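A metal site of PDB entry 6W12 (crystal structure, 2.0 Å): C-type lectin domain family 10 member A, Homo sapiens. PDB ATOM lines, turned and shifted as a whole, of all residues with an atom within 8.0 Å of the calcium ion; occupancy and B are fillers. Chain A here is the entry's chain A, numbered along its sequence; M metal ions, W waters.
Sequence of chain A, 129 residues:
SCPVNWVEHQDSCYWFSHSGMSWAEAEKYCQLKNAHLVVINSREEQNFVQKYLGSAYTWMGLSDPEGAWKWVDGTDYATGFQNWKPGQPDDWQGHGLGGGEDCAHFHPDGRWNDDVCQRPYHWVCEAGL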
ATOM      1  N   HIS A   9      31.863  22.901 -24.853  1.00  0.00           N
ATOM      2  CA  HIS A   9      31.662  24.247 -24.253  1.00  0.00           C
ATOM      3  C   HIS A   9      31.897  24.110 -22.743  1.00  0.00           C
ATOM      4  O   HIS A   9      31.165  23.323 -22.111  1.00  0.00           O
ATOM      5  CB  HIS A   9      30.296  24.829 -24.646  1.00  0.00           C
ATOM      6  CG  HIS A   9      29.974  26.146 -24.006  1.00  0.00           C
ATOM      7  ND1 HIS A   9      30.399  27.367 -24.540  1.00  0.00           N
ATOM      8  CD2 HIS A   9      29.304  26.457 -22.868  1.00  0.00           C
ATOM      9  CE1 HIS A   9      30.015  28.348 -23.737  1.00  0.00           C
ATOM     10  NE2 HIS A   9      29.339  27.826 -22.703  1.00  0.00           N
ATOM     11  N   GLN A  10      32.920  24.780 -22.202  1.00  0.00           N
ATOM     12  CA  GLN A  10      33.097  24.976 -20.732  1.00  0.00           C
ATOM     13  C   GLN A  10      32.943  23.648 -19.980  1.00  0.00           C
ATOM     14  O   GLN A  10      31.975  23.539 -19.180  1.00  0.00           O
ATOM     15  CB  GLN A  10      32.065  25.950 -20.148  1.00  0.00           C
ATOM     16  CG  GLN A  10      32.089  27.360 -20.731  1.00  0.00           C
ATOM     17  CD  GLN A  10      33.377  28.093 -20.476  1.00  0.00           C
ATOM     18  OE1 GLN A  10      33.833  28.212 -19.341  1.00  0.00           O
ATOM     19  NE2 GLN A  10      33.987  28.597 -21.544  1.00  0.00           N
ATOM     20  N   ASP A  11      33.811  22.668 -20.229  1.00  0.00           N
ATOM     21  CA  ASP A  11      33.846  21.421 -19.409  1.00  0.00           C
ATOM     22  C   ASP A  11      32.659  20.490 -19.664  1.00  0.00           C
ATOM     23  O   ASP A  11      32.548  19.531 -18.903  1.00  0.00           O
ATOM     24  CB  ASP A  11      33.859  21.709 -17.904  1.00  0.00           C
ATOM     25  CG  ASP A  11      35.209  22.238 -17.429  1.00  0.00           C
ATOM     26  OD1 ASP A  11      36.232  21.772 -17.972  1.00  0.00           O
ATOM     27  OD2 ASP A  11      35.212  23.107 -16.535  1.00  0.00           O
ATOM     28  N   SER A  12      31.803  20.724 -20.667  1.00  0.00           N
ATOM     29  CA  SER A  12      30.838  19.700 -21.123  1.00  0.00           C
ATOM     30  C   SER A  12      30.997  19.464 -22.632  1.00  0.00           C
ATOM     31  O   SER A  12      31.534  20.317 -23.316  1.00  0.00           O
ATOM     32  CB  SER A  12      29.422  20.096 -20.814  1.00  0.00           C
ATOM     33  OG  SER A  12      29.136  19.889 -19.454  1.00  0.00           O
ATOM     34  N   CYS A  13      30.578  18.290 -23.093  1.00  0.00           N
ATOM     35  CA  CYS A  13      30.420  17.944 -24.513  1.00  0.00           C
ATOM     36  C   CYS A  13      28.916  17.859 -24.753  1.00  0.00           C
ATOM     37  O   CYS A  13      28.226  17.319 -23.880  1.00  0.00           O
ATOM     38  CB  CYS A  13      31.035  16.591 -24.834  1.00  0.00           C
ATOM     39  SG  CYS A  13      32.818  16.594 -24.583  1.00  0.00           S
ATOM     40  N   TYR A  14      28.470  18.333 -25.906  1.00  0.00           N
ATOM     41  CA  TYR A  14      27.045  18.357 -26.271  1.00  0.00           C
ATOM     42  C   TYR A  14      26.886  17.726 -27.637  1.00  0.00           C
ATOM     43  O   TYR A  14      27.762  17.921 -28.504  1.00  0.00           O
ATOM     44  CB  TYR A  14      26.530  19.792 -26.323  1.00  0.00           C
ATOM     45  CG  TYR A  14      26.672  20.535 -25.026  1.00  0.00           C
ATOM     46  CD1 TYR A  14      27.861  21.097 -24.630  1.00  0.00           C
ATOM     47  CD2 TYR A  14      25.603  20.618 -24.150  1.00  0.00           C
ATOM     48  CE1 TYR A  14      27.988  21.767 -23.409  1.00  0.00           C
ATOM     49  CE2 TYR A  14      25.705  21.281 -22.944  1.00  0.00           C
ATOM     50  CZ  TYR A  14      26.898  21.878 -22.571  1.00  0.00           C
ATOM     51  OH  TYR A  14      26.968  22.510 -21.376  1.00  0.00           O
ATOM     52  N   HIS A  36      23.665  12.080 -20.955  1.00  0.00           N
ATOM     53  CA  HIS A  36      22.292  12.265 -20.447  1.00  0.00           C
ATOM     54  C   HIS A  36      21.671  13.441 -21.198  1.00  0.00           C
ATOM     55  O   HIS A  36      22.436  14.263 -21.737  1.00  0.00           O
ATOM     56  CB  HIS A  36      22.354  12.401 -18.905  1.00  0.00           C
ATOM     57  CG  HIS A  36      23.243  13.513 -18.435  1.00  0.00           C
ATOM     58  ND1 HIS A  36      22.918  14.849 -18.616  1.00  0.00           N
ATOM     59  CD2 HIS A  36      24.448  13.518 -17.811  1.00  0.00           C
ATOM     60  CE1 HIS A  36      23.899  15.618 -18.129  1.00  0.00           C
ATOM     61  NE2 HIS A  36      24.838  14.833 -17.603  1.00  0.00           N
ATOM     62  N   LEU A  37      20.355  13.528 -21.234  1.00  0.00           N
ATOM     63  CA  LEU A  37      19.668  14.730 -21.745  1.00  0.00           C
ATOM     64  C   LEU A  37      20.236  15.951 -21.018  1.00  0.00           C
ATOM     65  O   LEU A  37      20.559  15.884 -19.786  1.00  0.00           O
ATOM     66  CB  LEU A  37      18.154  14.611 -21.513  1.00  0.00           C
ATOM     67  CG  LEU A  37      17.365  13.725 -22.477  1.00  0.00           C
ATOM     68  CD1 LEU A  37      15.928  13.590 -22.013  1.00  0.00           C
ATOM     69  CD2 LEU A  37      17.420  14.257 -23.867  1.00  0.00           C
ATOM     70  N   VAL A  38      20.411  17.042 -21.778  1.00  0.00           N
ATOM     71  CA  VAL A  38      21.122  18.248 -21.290  1.00  0.00           C
ATOM     72  C   VAL A  38      20.471  18.711 -19.982  1.00  0.00           C
ATOM     73  O   VAL A  38      19.236  18.652 -19.831  1.00  0.00           O
ATOM     74  CB  VAL A  38      21.160  19.329 -22.374  1.00  0.00           C
ATOM     75  CG1 VAL A  38      19.758  19.846 -22.709  1.00  0.00           C
ATOM     76  CG2 VAL A  38      22.140  20.424 -22.017  1.00  0.00           C
ATOM     77  N   VAL A  39      21.305  19.087 -19.033  1.00  0.00           N
ATOM     78  CA  VAL A  39      20.908  19.694 -17.730  1.00  0.00           C
ATOM     79  C   VAL A  39      21.350  21.154 -17.832  1.00  0.00           C
ATOM     80  O   VAL A  39      22.540  21.350 -18.083  1.00  0.00           O
ATOM     81  CB  VAL A  39      21.591  18.986 -16.543  1.00  0.00           C
ATOM     82  CG1 VAL A  39      21.409  19.737 -15.242  1.00  0.00           C
ATOM     83  CG2 VAL A  39      21.091  17.556 -16.395  1.00  0.00           C
ATOM     84  N   ILE A  40      20.455  22.118 -17.650  1.00  0.00           N
ATOM     85  CA  ILE A  40      20.853  23.554 -17.747  1.00  0.00           C
ATOM     86  C   ILE A  40      21.178  24.053 -16.341  1.00  0.00           C
ATOM     87  O   ILE A  40      20.253  24.197 -15.534  1.00  0.00           O
ATOM     88  CB  ILE A  40      19.792  24.401 -18.474  1.00  0.00           C
ATOM     89  CG1 ILE A  40      19.394  23.814 -19.823  1.00  0.00           C
ATOM     90  CG2 ILE A  40      20.281  25.844 -18.618  1.00  0.00           C
ATOM     91  CD1 ILE A  40      20.475  23.882 -20.885  1.00  0.00           C
ATOM     92  N   ASN A  41      22.448  24.381 -16.084  1.00  0.00           N
ATOM     93  CA  ASN A  41      22.970  24.660 -14.736  1.00  0.00           C
ATOM     94  C   ASN A  41      23.088  26.172 -14.515  1.00  0.00           C
ATOM     95  O   ASN A  41      23.264  26.553 -13.400  1.00  0.00           O
ATOM     96  CB  ASN A  41      24.333  23.974 -14.504  1.00  0.00           C
ATOM     97  CG  ASN A  41      24.233  22.473 -14.575  1.00  0.00           C
ATOM     98  OD1 ASN A  41      24.361  21.902 -15.648  1.00  0.00           O
ATOM     99  ND2 ASN A  41      24.007  21.824 -13.440  1.00  0.00           N
ATOM    100  N   SER A  42      23.057  26.992 -15.576  1.00  0.00           N
ATOM    101  CA  SER A  42      23.414  28.441 -15.515  1.00  0.00           C
ATOM    102  C   SER A  42      22.824  29.159 -16.731  1.00  0.00           C
ATOM    103  O   SER A  42      22.609  28.490 -17.743  1.00  0.00           O
ATOM    104  CB  SER A  42      24.929  28.629 -15.453  1.00  0.00           C
ATOM    105  OG  SER A  42      25.523  28.197 -16.698  1.00  0.00           O
ATOM    106  N   GLU A  45      25.012  28.664 -19.775  1.00  0.00           N
ATOM    107  CA  GLU A  45      24.774  27.386 -20.503  1.00  0.00           C
ATOM    108  C   GLU A  45      23.462  27.488 -21.289  1.00  0.00           C
ATOM    109  O   GLU A  45      23.408  26.976 -22.432  1.00  0.00           O
ATOM    110  CB  GLU A  45      24.765  26.206 -19.540  1.00  0.00           C
ATOM    111  CG  GLU A  45      24.471  24.893 -20.214  1.00  0.00           C
ATOM    112  CD  GLU A  45      24.660  23.709 -19.295  1.00  0.00           C
ATOM    113  OE1 GLU A  45      24.432  23.914 -18.110  1.00  0.00           O
ATOM    114  OE2 GLU A  45      25.088  22.583 -19.781  1.00  0.00           O
ATOM    115  N   GLN A  46      22.425  28.096 -20.697  1.00  0.00           N
ATOM    116  CA  GLN A  46      21.144  28.345 -21.378  1.00  0.00           C
ATOM    117  C   GLN A  46      21.456  29.122 -22.676  1.00  0.00           C
ATOM    118  O   GLN A  46      20.946  28.741 -23.723  1.00  0.00           O
ATOM    119  CB  GLN A  46      20.190  29.071 -20.433  1.00  0.00           C
ATOM    120  CG  GLN A  46      18.959  29.614 -21.124  1.00  0.00           C
ATOM    121  CD  GLN A  46      18.014  28.535 -21.579  1.00  0.00           C
ATOM    122  OE1 GLN A  46      17.709  27.594 -20.847  1.00  0.00           O
ATOM    123  NE2 GLN A  46      17.478  28.726 -22.784  1.00  0.00           N
ATOM    124  N   VAL A  49      23.247  26.819 -25.358  1.00  0.00           N
ATOM    125  CA  VAL A  49      22.312  25.819 -25.947  1.00  0.00           C
ATOM    126  C   VAL A  49      21.307  26.539 -26.845  1.00  0.00           C
ATOM    127  O   VAL A  49      21.051  26.046 -27.946  1.00  0.00           O
ATOM    128  CB  VAL A  49      21.613  24.992 -24.856  1.00  0.00           C
ATOM    129  CG1 VAL A  49      20.534  24.099 -25.448  1.00  0.00           C
ATOM    130  CG2 VAL A  49      22.613  24.163 -24.058  1.00  0.00           C
ATOM    131  N   TRP A  71      16.053  16.946 -12.411  1.00  0.00           N
ATOM    132  CA  TRP A  71      17.028  16.846 -13.514  1.00  0.00           C
ATOM    133  C   TRP A  71      17.578  15.426 -13.577  1.00  0.00           C
ATOM    134  O   TRP A  71      17.748  14.789 -12.527  1.00  0.00           O
ATOM    135  CB  TRP A  71      18.124  17.864 -13.326  1.00  0.00           C
ATOM    136  CG  TRP A  71      17.716  19.289 -13.516  1.00  0.00           C
ATOM    137  CD1 TRP A  71      17.539  20.217 -12.534  1.00  0.00           C
ATOM    138  CD2 TRP A  71      17.588  20.012 -14.756  1.00  0.00           C
ATOM    139  NE1 TRP A  71      17.264  21.433 -13.080  1.00  0.00           N
ATOM    140  CE2 TRP A  71      17.286  21.348 -14.436  1.00  0.00           C
ATOM    141  CE3 TRP A  71      17.635  19.634 -16.105  1.00  0.00           C
ATOM    142  CZ2 TRP A  71      17.075  22.323 -15.411  1.00  0.00           C
ATOM    143  CZ3 TRP A  71      17.395  20.589 -17.070  1.00  0.00           C
ATOM    144  CH2 TRP A  71      17.145  21.924 -16.734  1.00  0.00           C
ATOM    145  N   ASP A  73      20.417  14.089 -13.899  1.00  0.00           N
ATOM    146  CA  ASP A  73      21.715  13.804 -13.249  1.00  0.00           C
ATOM    147  C   ASP A  73      21.663  14.073 -11.732  1.00  0.00           C
ATOM    148  O   ASP A  73      22.680  13.858 -11.066  1.00  0.00           O
ATOM    149  CB  ASP A  73      22.845  14.539 -13.956  1.00  0.00           C
ATOM    150  CG  ASP A  73      22.965  16.010 -13.612  1.00  0.00           C
ATOM    151  OD1 ASP A  73      21.980  16.593 -13.071  1.00  0.00           O
ATOM    152  OD2 ASP A  73      24.063  16.569 -13.895  1.00  0.00           O
ATOM    153  N   THR A  75      20.920  17.160 -10.386  1.00  0.00           N
ATOM    154  CA  THR A  75      21.027  18.616 -10.074  1.00  0.00           C
ATOM    155  C   THR A  75      19.724  19.064  -9.416  1.00  0.00           C
ATOM    156  O   THR A  75      18.624  18.642  -9.843  1.00  0.00           O
ATOM    157  CB  THR A  75      21.286  19.413 -11.356  1.00  0.00           C
ATOM    158  OG1 THR A  75      22.555  18.998 -11.877  1.00  0.00           O
ATOM    159  CG2 THR A  75      21.256  20.905 -11.142  1.00  0.00           C
ATOM    160  N   GLU A 126      24.381  15.653 -23.165  1.00  0.00           N
ATOM    161  CA  GLU A 126      25.505  16.335 -22.485  1.00  0.00           C
ATOM    162  C   GLU A 126      26.293  15.261 -21.740  1.00  0.00           C
ATOM    163  O   GLU A 126      25.669  14.324 -21.203  1.00  0.00           O
ATOM    164  CB  GLU A 126      24.992  17.398 -21.512  1.00  0.00           C
ATOM    165  CG  GLU A 126      26.092  18.213 -20.828  1.00  0.00           C
ATOM    166  CD  GLU A 126      25.606  19.221 -19.767  1.00  0.00           C
ATOM    167  OE1 GLU A 126      24.394  19.236 -19.434  1.00  0.00           O
ATOM    168  OE2 GLU A 126      26.452  20.033 -19.279  1.00  0.00           O
ATOM    169  N   ALA A 127      27.621  15.401 -21.721  1.00  0.00           N
ATOM    170  CA  ALA A 127      28.518  14.575 -20.890  1.00  0.00           C
ATOM    171  C   ALA A 127      29.671  15.444 -20.385  1.00  0.00           C
ATOM    172  O   ALA A 127      30.049  16.380 -21.062  1.00  0.00           O
ATOM    173  CB  ALA A 127      29.003  13.378 -21.678  1.00  0.00           C
HETATM  174 CA    CA M   1      24.926  21.269 -17.838  1.00  0.00          CA
HETATM  175 ZN    ZN M   2      26.567  15.224 -16.782  1.00  0.00          ZN
HETATM  176  O   HOH W   1      25.388  19.329 -16.581  1.00  0.00           O
HETATM  177  O   HOH W   2      26.987  22.285 -17.160  1.00  0.00           O
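The side-chain carboxylate (OE2) of Glu 126 sits close to the side-chain hydroxyl (OH) of Tyr 14.
The backbone NH (N) of Glu 45 is in hydrogen-bond range of the side-chain hydroxyl (OG) of Ser 42 (3.2 Å).
OH of Tyr 14 sits close to OE2 of Glu 45 (2.5 Å).
The side-chain carboxylate of Glu 126 lies close to the side-chain hydroxyl of Ser 12 (2.7 Å).
N of Glu 126 sits at hydrogen-bond distance from O of His 36 (2.8 Å).
Of the 21 residues printed, 4 come within 4 Å of the calcium ion.
The nearest printed residue that does not touch the calcium ion is Tyr 14 (4.3 Å).
The calcium ion is bound by OD1 of Asn 41 (2.3 Å), OE2 of Glu 45 (2.4 Å), water W1 (2.4 Å), water W2 (2.4 Å), O of Val 39 (2.4 Å), OE2 of Glu 126 (2.4 Å), OE1 of Glu 126 (2.6 Å) and OE1 of Glu 45 (2.7 Å).
The calcium ion has eight donor atoms within binding distance.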
